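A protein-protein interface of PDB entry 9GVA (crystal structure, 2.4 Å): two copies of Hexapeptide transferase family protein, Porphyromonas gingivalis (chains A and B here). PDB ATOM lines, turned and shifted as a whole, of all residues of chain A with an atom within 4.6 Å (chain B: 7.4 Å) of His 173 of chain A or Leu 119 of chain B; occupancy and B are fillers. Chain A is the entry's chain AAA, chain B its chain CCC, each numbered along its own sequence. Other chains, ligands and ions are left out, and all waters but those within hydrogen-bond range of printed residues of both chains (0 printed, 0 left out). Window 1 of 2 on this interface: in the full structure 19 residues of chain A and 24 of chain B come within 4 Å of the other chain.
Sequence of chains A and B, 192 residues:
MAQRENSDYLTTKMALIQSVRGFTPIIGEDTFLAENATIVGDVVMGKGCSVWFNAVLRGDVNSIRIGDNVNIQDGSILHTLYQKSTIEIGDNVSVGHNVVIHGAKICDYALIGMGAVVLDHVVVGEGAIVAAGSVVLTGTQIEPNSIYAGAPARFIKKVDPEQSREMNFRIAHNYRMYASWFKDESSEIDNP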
ATOM      1  N   MET A 114       3.585  -6.065   2.314  1.00  0.00           N
ATOM      2  CA  MET A 114       3.673  -5.589   0.923  1.00  0.00           C
ATOM      3  C   MET A 114       3.361  -6.731  -0.043  1.00  0.00           C
ATOM      4  O   MET A 114       3.818  -7.851   0.154  1.00  0.00           O
ATOM      5  CB  MET A 114       5.042  -4.979   0.642  1.00  0.00           C
ATOM      6  CG  MET A 114       6.193  -5.946   0.702  1.00  0.00           C
ATOM      7  SD  MET A 114       7.729  -4.998   1.020  1.00  0.00           S
ATOM      8  CE  MET A 114       7.580  -4.854   2.801  1.00  0.00           C
ATOM      9  N   ALA A 131       1.808 -11.888   6.068  1.00  0.00           N
ATOM     10  CA  ALA A 131       3.158 -11.771   5.501  1.00  0.00           C
ATOM     11  C   ALA A 131       3.095 -11.238   4.061  1.00  0.00           C
ATOM     12  O   ALA A 131       2.050 -11.354   3.385  1.00  0.00           O
ATOM     13  CB  ALA A 131       3.799 -13.107   5.573  1.00  0.00           C
ATOM     14  N   ALA A 132       4.211 -10.673   3.594  1.00  0.00           N
ATOM     15  CA  ALA A 132       4.363 -10.085   2.252  1.00  0.00           C
ATOM     16  C   ALA A 132       3.935 -11.127   1.212  1.00  0.00           C
ATOM     17  O   ALA A 132       4.267 -12.280   1.393  1.00  0.00           O
ATOM     18  CB  ALA A 132       5.790  -9.653   2.065  1.00  0.00           C
ATOM     19  N   PHE A 169       7.037  -8.687  12.674  1.00  0.00           N
ATOM     20  CA  PHE A 169       6.998  -8.529  11.198  1.00  0.00           C
ATOM     21  C   PHE A 169       8.317  -9.030  10.604  1.00  0.00           C
ATOM     22  O   PHE A 169       8.278  -9.952   9.754  1.00  0.00           O
ATOM     23  CB  PHE A 169       6.686  -7.078  10.802  1.00  0.00           C
ATOM     24  CG  PHE A 169       6.283  -6.936   9.360  1.00  0.00           C
ATOM     25  CD1 PHE A 169       7.245  -6.777   8.374  1.00  0.00           C
ATOM     26  CD2 PHE A 169       4.948  -6.997   8.985  1.00  0.00           C
ATOM     27  CE1 PHE A 169       6.887  -6.663   7.036  1.00  0.00           C
ATOM     28  CE2 PHE A 169       4.593  -6.876   7.653  1.00  0.00           C
ATOM     29  CZ  PHE A 169       5.561  -6.705   6.683  1.00  0.00           C
ATOM     30  N   ARG A 170       9.446  -8.472  11.055  1.00  0.00           N
ATOM     31  CA  ARG A 170      10.803  -8.790  10.531  1.00  0.00           C
ATOM     32  C   ARG A 170      11.066 -10.303  10.655  1.00  0.00           C
ATOM     33  O   ARG A 170      11.585 -10.907   9.683  1.00  0.00           O
ATOM     34  CB  ARG A 170      11.885  -7.993  11.271  1.00  0.00           C
ATOM     35  CG  ARG A 170      12.047  -6.547  10.822  1.00  0.00           C
ATOM     36  CD  ARG A 170      13.419  -5.955  11.113  1.00  0.00           C
ATOM     37  NE  ARG A 170      13.309  -4.535  10.837  1.00  0.00           N
ATOM     38  CZ  ARG A 170      12.812  -3.630  11.683  1.00  0.00           C
ATOM     39  NH1 ARG A 170      12.429  -3.985  12.899  1.00  0.00           N
ATOM     40  NH2 ARG A 170      12.711  -2.365  11.314  1.00  0.00           N
ATOM     41  N   ILE A 171      10.721 -10.894  11.796  1.00  0.00           N
ATOM     42  CA  ILE A 171      10.946 -12.342  12.078  1.00  0.00           C
ATOM     43  C   ILE A 171      10.102 -13.185  11.103  1.00  0.00           C
ATOM     44  O   ILE A 171      10.650 -14.198  10.596  1.00  0.00           O
ATOM     45  CB  ILE A 171      10.643 -12.661  13.566  1.00  0.00           C
ATOM     46  CG1 ILE A 171      11.627 -11.974  14.521  1.00  0.00           C
ATOM     47  CG2 ILE A 171      10.600 -14.163  13.824  1.00  0.00           C
ATOM     48  CD1 ILE A 171      11.099 -11.821  15.921  1.00  0.00           C
ATOM     49  N   ALA A 172       8.831 -12.799  10.878  1.00  0.00           N
ATOM     50  CA  ALA A 172       7.849 -13.410   9.932  1.00  0.00           C
ATOM     51  C   ALA A 172       8.322 -13.361   8.468  1.00  0.00           C
ATOM     52  O   ALA A 172       7.751 -14.133   7.657  1.00  0.00           O
ATOM     53  CB  ALA A 172       6.491 -12.730  10.036  1.00  0.00           C
ATOM     54  N   HIS A 173       9.263 -12.465   8.132  1.00  0.00           N
ATOM     55  CA  HIS A 173       9.798 -12.263   6.759  1.00  0.00           C
ATOM     56  C   HIS A 173      11.244 -12.748   6.634  1.00  0.00           C
ATOM     57  O   HIS A 173      11.867 -12.484   5.579  1.00  0.00           O
ATOM     58  CB  HIS A 173       9.584 -10.809   6.375  1.00  0.00           C
ATOM     59  CG  HIS A 173       8.146 -10.547   6.087  1.00  0.00           C
ATOM     60  ND1 HIS A 173       7.314  -9.880   6.968  1.00  0.00           N
ATOM     61  CD2 HIS A 173       7.375 -10.931   5.055  1.00  0.00           C
ATOM     62  CE1 HIS A 173       6.104  -9.832   6.466  1.00  0.00           C
ATOM     63  NE2 HIS A 173       6.112 -10.494   5.311  1.00  0.00           N
ATOM     64  N   ASN A 174      11.731 -13.480   7.636  1.00  0.00           N
ATOM     65  CA  ASN A 174      13.101 -14.052   7.638  1.00  0.00           C
ATOM     66  C   ASN A 174      13.023 -15.534   7.238  1.00  0.00           C
ATOM     67  O   ASN A 174      12.106 -16.233   7.725  1.00  0.00           O
ATOM     68  CB  ASN A 174      13.792 -13.833   8.986  1.00  0.00           C
ATOM     69  CG  ASN A 174      15.278 -14.081   8.875  1.00  0.00           C
ATOM     70  OD1 ASN A 174      15.711 -15.214   8.713  1.00  0.00           O
ATOM     71  ND2 ASN A 174      16.066 -13.022   8.896  1.00  0.00           N
ATOM     72  N   TYR A 175      13.940 -15.992   6.381  1.00  0.00           N
ATOM     73  CA  TYR A 175      13.938 -17.372   5.830  1.00  0.00           C
ATOM     74  C   TYR A 175      14.109 -18.383   6.975  1.00  0.00           C
ATOM     75  O   TYR A 175      13.567 -19.493   6.847  1.00  0.00           O
ATOM     76  CB  TYR A 175      14.987 -17.556   4.722  1.00  0.00           C
ATOM     77  CG  TYR A 175      14.850 -18.863   3.975  1.00  0.00           C
ATOM     78  CD1 TYR A 175      15.382 -20.037   4.494  1.00  0.00           C
ATOM     79  CD2 TYR A 175      14.153 -18.944   2.776  1.00  0.00           C
ATOM     80  CE1 TYR A 175      15.244 -21.250   3.838  1.00  0.00           C
ATOM     81  CE2 TYR A 175      14.004 -20.148   2.106  1.00  0.00           C
ATOM     82  CZ  TYR A 175      14.553 -21.302   2.640  1.00  0.00           C
ATOM     83  OH  TYR A 175      14.419 -22.494   1.991  1.00  0.00           O
ATOM     84  N   GLU A 185       5.486 -17.767   2.870  1.00  0.00           N
ATOM     85  CA  GLU A 185       6.306 -16.518   2.984  1.00  0.00           C
ATOM     86  C   GLU A 185       6.515 -16.143   4.449  1.00  0.00           C
ATOM     87  O   GLU A 185       6.714 -14.955   4.713  1.00  0.00           O
ATOM     88  CB  GLU A 185       5.693 -15.264   2.359  1.00  0.00           C
ATOM     89  CG  GLU A 185       5.194 -15.455   0.948  1.00  0.00           C
ATOM     90  CD  GLU A 185       3.683 -15.423   0.838  1.00  0.00           C
ATOM     91  OE1 GLU A 185       3.136 -15.800  -0.239  1.00  0.00           O
ATOM     92  OE2 GLU A 185       3.062 -15.016   1.829  1.00  0.00           O
ATOM     93  N   SER B  85      17.775  -0.364   6.746  1.00  0.00           N
ATOM     94  CA  SER B  85      18.110  -0.933   5.410  1.00  0.00           C
ATOM     95  C   SER B  85      18.223   0.168   4.350  1.00  0.00           C
ATOM     96  O   SER B  85      17.720   1.287   4.540  1.00  0.00           O
ATOM     97  CB  SER B  85      17.089  -1.990   5.009  1.00  0.00           C
ATOM     98  OG  SER B  85      15.790  -1.390   4.828  1.00  0.00           O
ATOM     99  N   VAL B 100       8.026  -4.881  -5.831  1.00  0.00           N
ATOM    100  CA  VAL B 100       8.458  -4.131  -4.610  1.00  0.00           C
ATOM    101  C   VAL B 100       9.874  -4.572  -4.211  1.00  0.00           C
ATOM    102  O   VAL B 100      10.107  -5.771  -3.975  1.00  0.00           O
ATOM    103  CB  VAL B 100       7.480  -4.307  -3.446  1.00  0.00           C
ATOM    104  CG1 VAL B 100       7.934  -3.459  -2.257  1.00  0.00           C
ATOM    105  CG2 VAL B 100       6.044  -3.990  -3.870  1.00  0.00           C
ATOM    106  N   ILE B 101      10.774  -3.604  -4.132  1.00  0.00           N
ATOM    107  CA  ILE B 101      12.151  -3.774  -3.608  1.00  0.00           C
ATOM    108  C   ILE B 101      12.238  -2.959  -2.325  1.00  0.00           C
ATOM    109  O   ILE B 101      12.037  -1.733  -2.387  1.00  0.00           O
ATOM    110  CB  ILE B 101      13.161  -3.366  -4.698  1.00  0.00           C
ATOM    111  CG1 ILE B 101      13.105  -4.403  -5.825  1.00  0.00           C
ATOM    112  CG2 ILE B 101      14.561  -3.258  -4.125  1.00  0.00           C
ATOM    113  CD1 ILE B 101      13.665  -3.930  -7.106  1.00  0.00           C
ATOM    114  N   HIS B 102      12.411  -3.652  -1.195  1.00  0.00           N
ATOM    115  CA  HIS B 102      12.494  -3.087   0.183  1.00  0.00           C
ATOM    116  C   HIS B 102      13.875  -3.410   0.762  1.00  0.00           C
ATOM    117  O   HIS B 102      14.110  -4.582   1.065  1.00  0.00           O
ATOM    118  CB  HIS B 102      11.363  -3.636   1.050  1.00  0.00           C
ATOM    119  CG  HIS B 102      10.739  -2.620   1.934  1.00  0.00           C
ATOM    120  ND1 HIS B 102      11.248  -2.341   3.178  1.00  0.00           N
ATOM    121  CD2 HIS B 102       9.695  -1.785   1.732  1.00  0.00           C
ATOM    122  CE1 HIS B 102      10.532  -1.365   3.718  1.00  0.00           C
ATOM    123  NE2 HIS B 102       9.562  -1.003   2.837  1.00  0.00           N
ATOM    124  N   GLY B 103      14.795  -2.444   0.742  1.00  0.00           N
ATOM    125  CA  GLY B 103      16.073  -2.469   1.486  1.00  0.00           C
ATOM    126  C   GLY B 103      17.005  -3.574   1.013  1.00  0.00           C
ATOM    127  O   GLY B 103      17.664  -4.199   1.837  1.00  0.00           O
ATOM    128  N   ALA B 104      17.015  -3.829  -0.282  1.00  0.00           N
ATOM    129  CA  ALA B 104      17.759  -4.940  -0.894  1.00  0.00           C
ATOM    130  C   ALA B 104      18.931  -4.376  -1.684  1.00  0.00           C
ATOM    131  O   ALA B 104      18.875  -3.214  -2.113  1.00  0.00           O
ATOM    132  CB  ALA B 104      16.853  -5.742  -1.795  1.00  0.00           C
ATOM    133  N   LYS B 105      19.937  -5.221  -1.874  1.00  0.00           N
ATOM    134  CA  LYS B 105      21.056  -4.985  -2.788  1.00  0.00           C
ATOM    135  C   LYS B 105      20.923  -5.909  -4.003  1.00  0.00           C
ATOM    136  O   LYS B 105      20.746  -7.124  -3.835  1.00  0.00           O
ATOM    137  CB  LYS B 105      22.312  -5.233  -1.970  1.00  0.00           C
ATOM    138  CG  LYS B 105      23.590  -4.972  -2.729  1.00  0.00           C
ATOM    139  CD  LYS B 105      24.776  -5.535  -1.996  1.00  0.00           C
ATOM    140  CE  LYS B 105      26.058  -5.301  -2.749  1.00  0.00           C
ATOM    141  NZ  LYS B 105      26.168  -3.853  -3.060  1.00  0.00           N
ATOM    142  N   VAL B 117       8.375  -9.548  -4.938  1.00  0.00           N
ATOM    143  CA  VAL B 117       8.680  -8.783  -3.697  1.00  0.00           C
ATOM    144  C   VAL B 117      10.067  -9.233  -3.204  1.00  0.00           C
ATOM    145  O   VAL B 117      10.268 -10.449  -2.957  1.00  0.00           O
ATOM    146  CB  VAL B 117       7.592  -9.025  -2.634  1.00  0.00           C
ATOM    147  CG1 VAL B 117       7.916  -8.326  -1.311  1.00  0.00           C
ATOM    148  CG2 VAL B 117       6.229  -8.619  -3.167  1.00  0.00           C
ATOM    149  N   VAL B 118      10.990  -8.290  -3.049  1.00  0.00           N
ATOM    150  CA  VAL B 118      12.380  -8.577  -2.599  1.00  0.00           C
ATOM    151  C   VAL B 118      12.565  -7.792  -1.312  1.00  0.00           C
ATOM    152  O   VAL B 118      12.481  -6.561  -1.372  1.00  0.00           O
ATOM    153  CB  VAL B 118      13.443  -8.190  -3.631  1.00  0.00           C
ATOM    154  CG1 VAL B 118      14.817  -8.572  -3.125  1.00  0.00           C
ATOM    155  CG2 VAL B 118      13.215  -8.794  -5.005  1.00  0.00           C
ATOM    156  N   LEU B 119      12.755  -8.487  -0.193  1.00  0.00           N
ATOM    157  CA  LEU B 119      12.731  -7.876   1.159  1.00  0.00           C
ATOM    158  C   LEU B 119      14.142  -7.471   1.650  1.00  0.00           C
ATOM    159  O   LEU B 119      15.145  -7.626   0.899  1.00  0.00           O
ATOM    160  CB  LEU B 119      12.012  -8.852   2.085  1.00  0.00           C
ATOM    161  CG  LEU B 119      10.536  -9.047   1.749  1.00  0.00           C
ATOM    162  CD1 LEU B 119       9.958 -10.162   2.577  1.00  0.00           C
ATOM    163  CD2 LEU B 119       9.743  -7.773   1.968  1.00  0.00           C
ATOM    164  N   ASP B 120      14.187  -6.858   2.836  1.00  0.00           N
ATOM    165  CA  ASP B 120      15.368  -6.128   3.374  1.00  0.00           C
ATOM    166  C   ASP B 120      16.513  -7.114   3.616  1.00  0.00           C
ATOM    167  O   ASP B 120      16.251  -8.277   4.019  1.00  0.00           O
ATOM    168  CB  ASP B 120      14.967  -5.324   4.609  1.00  0.00           C
ATOM    169  CG  ASP B 120      13.701  -4.514   4.375  1.00  0.00           C
ATOM    170  OD1 ASP B 120      13.806  -3.336   3.952  1.00  0.00           O
ATOM    171  OD2 ASP B 120      12.609  -5.107   4.537  1.00  0.00           O
ATOM    172  N   HIS B 121      17.738  -6.657   3.364  1.00  0.00           N
ATOM    173  CA  HIS B 121      19.018  -7.393   3.598  1.00  0.00           C
ATOM    174  C   HIS B 121      19.137  -8.560   2.622  1.00  0.00           C
ATOM    175  O   HIS B 121      19.995  -9.426   2.824  1.00  0.00           O
ATOM    176  CB  HIS B 121      19.138  -7.839   5.058  1.00  0.00           C
ATOM    177  CG  HIS B 121      18.867  -6.715   5.982  1.00  0.00           C
ATOM    178  ND1 HIS B 121      19.607  -5.533   5.919  1.00  0.00           N
ATOM    179  CD2 HIS B 121      17.901  -6.522   6.899  1.00  0.00           C
ATOM    180  CE1 HIS B 121      19.129  -4.671   6.790  1.00  0.00           C
ATOM    181  NE2 HIS B 121      18.088  -5.257   7.411  1.00  0.00           N
ATOM    182  N   VAL B 122      18.285  -8.605   1.606  1.00  0.00           N
ATOM    183  CA  VAL B 122      18.484  -9.572   0.492  1.00  0.00           C
ATOM    184  C   VAL B 122      19.646  -9.062  -0.361  1.00  0.00           C
ATOM    185  O   VAL B 122      19.778  -7.834  -0.607  1.00  0.00           O
ATOM    186  CB  VAL B 122      17.186  -9.776  -0.318  1.00  0.00           C
ATOM    187  CG1 VAL B 122      17.425 -10.513  -1.629  1.00  0.00           C
ATOM    188  CG2 VAL B 122      16.115 -10.465   0.533  1.00  0.00           C
ATOM    189  N   VAL B 123      20.435  -9.995  -0.853  1.00  0.00           N
ATOM    190  CA  VAL B 123      21.503  -9.675  -1.830  1.00  0.00           C
ATOM    191  C   VAL B 123      21.222 -10.531  -3.050  1.00  0.00           C
ATOM    192  O   VAL B 123      21.278 -11.763  -2.921  1.00  0.00           O
ATOM    193  CB  VAL B 123      22.917  -9.955  -1.276  1.00  0.00           C
ATOM    194  CG1 VAL B 123      23.940  -9.834  -2.384  1.00  0.00           C
ATOM    195  CG2 VAL B 123      23.272  -9.075  -0.083  1.00  0.00           C
ATOM    196  N   VAL B 135       8.488 -14.188  -3.737  1.00  0.00           N
ATOM    197  CA  VAL B 135       8.743 -13.391  -2.512  1.00  0.00           C
ATOM    198  C   VAL B 135      10.086 -13.838  -1.931  1.00  0.00           C
ATOM    199  O   VAL B 135      10.181 -14.967  -1.381  1.00  0.00           O
ATOM    200  CB  VAL B 135       7.558 -13.540  -1.552  1.00  0.00           C
ATOM    201  CG1 VAL B 135       7.715 -12.668  -0.328  1.00  0.00           C
ATOM    202  CG2 VAL B 135       6.258 -13.250  -2.306  1.00  0.00           C
ATOM    203  N   VAL B 136      11.112 -12.995  -2.088  1.00  0.00           N
ATOM    204  CA  VAL B 136      12.443 -13.252  -1.484  1.00  0.00           C
ATOM    205  C   VAL B 136      12.484 -12.752  -0.042  1.00  0.00           C
ATOM    206  O   VAL B 136      12.426 -11.519   0.202  1.00  0.00           O
ATOM    207  CB  VAL B 136      13.546 -12.645  -2.340  1.00  0.00           C
ATOM    208  CG1 VAL B 136      14.875 -13.220  -1.896  1.00  0.00           C
ATOM    209  CG2 VAL B 136      13.291 -12.928  -3.808  1.00  0.00           C
ATOM    210  N   LEU B 137      12.581 -13.672   0.904  1.00  0.00           N
ATOM    211  CA  LEU B 137      12.601 -13.304   2.345  1.00  0.00           C
ATOM    212  C   LEU B 137      13.934 -12.680   2.775  1.00  0.00           C
ATOM    213  O   LEU B 137      14.964 -12.914   2.111  1.00  0.00           O
ATOM    214  CB  LEU B 137      12.334 -14.568   3.137  1.00  0.00           C
ATOM    215  CG  LEU B 137      10.954 -15.180   2.906  1.00  0.00           C
ATOM    216  CD1 LEU B 137      10.781 -16.340   3.857  1.00  0.00           C
ATOM    217  CD2 LEU B 137       9.841 -14.148   3.095  1.00  0.00           C
ATOM    218  N   THR B 138      13.876 -11.882   3.844  1.00  0.00           N
ATOM    219  CA  THR B 138      15.026 -11.199   4.482  1.00  0.00           C
ATOM    220  C   THR B 138      16.193 -12.174   4.605  1.00  0.00           C
ATOM    221  O   THR B 138      15.939 -13.375   4.945  1.00  0.00           O
ATOM    222  CB  THR B 138      14.671 -10.672   5.874  1.00  0.00           C
ATOM    223  OG1 THR B 138      13.807  -9.552   5.675  1.00  0.00           O
ATOM    224  CG2 THR B 138      15.886 -10.272   6.682  1.00  0.00           C
ATOM    225  N   GLY B 139      17.401 -11.642   4.386  1.00  0.00           N
ATOM    226  CA  GLY B 139      18.674 -12.381   4.348  1.00  0.00           C
ATOM    227  C   GLY B 139      18.511 -13.671   3.575  1.00  0.00           C
ATOM    228  O   GLY B 139      18.752 -14.766   4.156  1.00  0.00           O
ATOM    229  N   THR B 140      17.979 -13.558   2.358  1.00  0.00           N
ATOM    230  CA  THR B 140      18.230 -14.534   1.276  1.00  0.00           C
ATOM    231  C   THR B 140      19.441 -13.970   0.527  1.00  0.00           C
ATOM    232  O   THR B 140      19.469 -12.737   0.270  1.00  0.00           O
ATOM    233  CB  THR B 140      16.997 -14.834   0.410  1.00  0.00           C
ATOM    234  OG1 THR B 140      15.858 -15.240   1.183  1.00  0.00           O
ATOM    235  CG2 THR B 140      17.334 -15.918  -0.583  1.00  0.00           C
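NE2 of His 173 of chain A lies within hydrogen-bond range of N of Ala 132 of chain A, at 2.6 Å.
The backbone carbonyl oxygen (O) of Phe 169 of chain A sits at hydrogen-bond distance from a ring nitrogen (ND1) of His 173 of chain A, at 2.9 Å.
The backbone NH of Val 118 of chain B sits at hydrogen-bond distance from the backbone carbonyl oxygen of Val 100 of chain B (2.8 Å).
The backbone carbonyl oxygen (O) of Val 117 of chain B lies within hydrogen-bond range of the backbone NH (N) of Val 136 of chain B.
N of Leu 119 of chain B lies within hydrogen-bond range of O of Val 136 of chain B, 3.1 Å away.
OG1 of Thr 138 of chain B lies close to O of Asp 120 of chain B (3.2 Å).
Of the 11 printed residues of chain A, 6 touch a printed residue of chain B.
Printed residues of chain A that touch a printed residue of chain B: Met 114, Ala 132, His 173, Asn 174, Tyr 175 and Glu 185.
Among the printed residues, 13 pairs touch across the chains.
Among the printed residues, no Asp or Glu carboxylate lies within 4 Å of a Lys or Arg side-chain nitrogen of the other chain.
Of chain B, only Leu 119 (3.7 Å), Leu 137 (3.2 Å) and Thr 138 (2.7 Å) come within 4 Å of His 173 of chain A.
Of chain A, only Met 114 (3.6 Å) and His 173 (3.7 Å) come within 4 Å of Leu 119 of chain B.
Printed residues of chain B within 4 Å of Glu 185 of chain A: Val 135 (3.9 Å) and Leu 137 (3.6 Å).
Printed residues of chain A within 4 Å of Val 135 of chain B: Ala 132 and Glu 185.
Printed residues of chain A within 4 Å of Thr 138 of chain B: His 173, Asn 174 and Tyr 175.
Of the printed residues of chain B, Ala 132 of chain A touches Val 135 (3.9 Å).
The nearest printed residue of chain B that does not touch Asn 174 of chain A is Leu 137 of chain B (4.1 Å).
Val 100 of chain B touches Met 114 of chain A (CG1 to SD, 3.6 Å).
His 102 of chain B touches Met 114 of chain A.
CG1 of Val 117 of chain B touches CG of Met 114 of chain A (3.6 Å).
Ala 132 of chain A touches Val 135 of chain B (O to CG1, 3.9 Å).
His 173 of chain A touches Leu 119 of chain B.
His 173 of chain A touches Leu 137 of chain B (O to CB, 3.2 Å).
Asn 174 of chain A touches Thr 138 of chain B.
Tyr 175 of chain A touches Leu 137 of chain B (CA to CD1, 3.9 Å).
Glu 185 of chain A touches Val 135 of chain B.
Leu 137 of chain B touches Glu 185 of chain A.
No position is printed for both chains.
Of the 13 pairs that touch across the chains among the printed residues, none has its exchanged pair printed and touching as well.
The backbone carbonyl oxygen (O) of His 173 of chain A lies within hydrogen-bond range of the backbone NH (N) of Thr 138 of chain B (2.7 Å).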
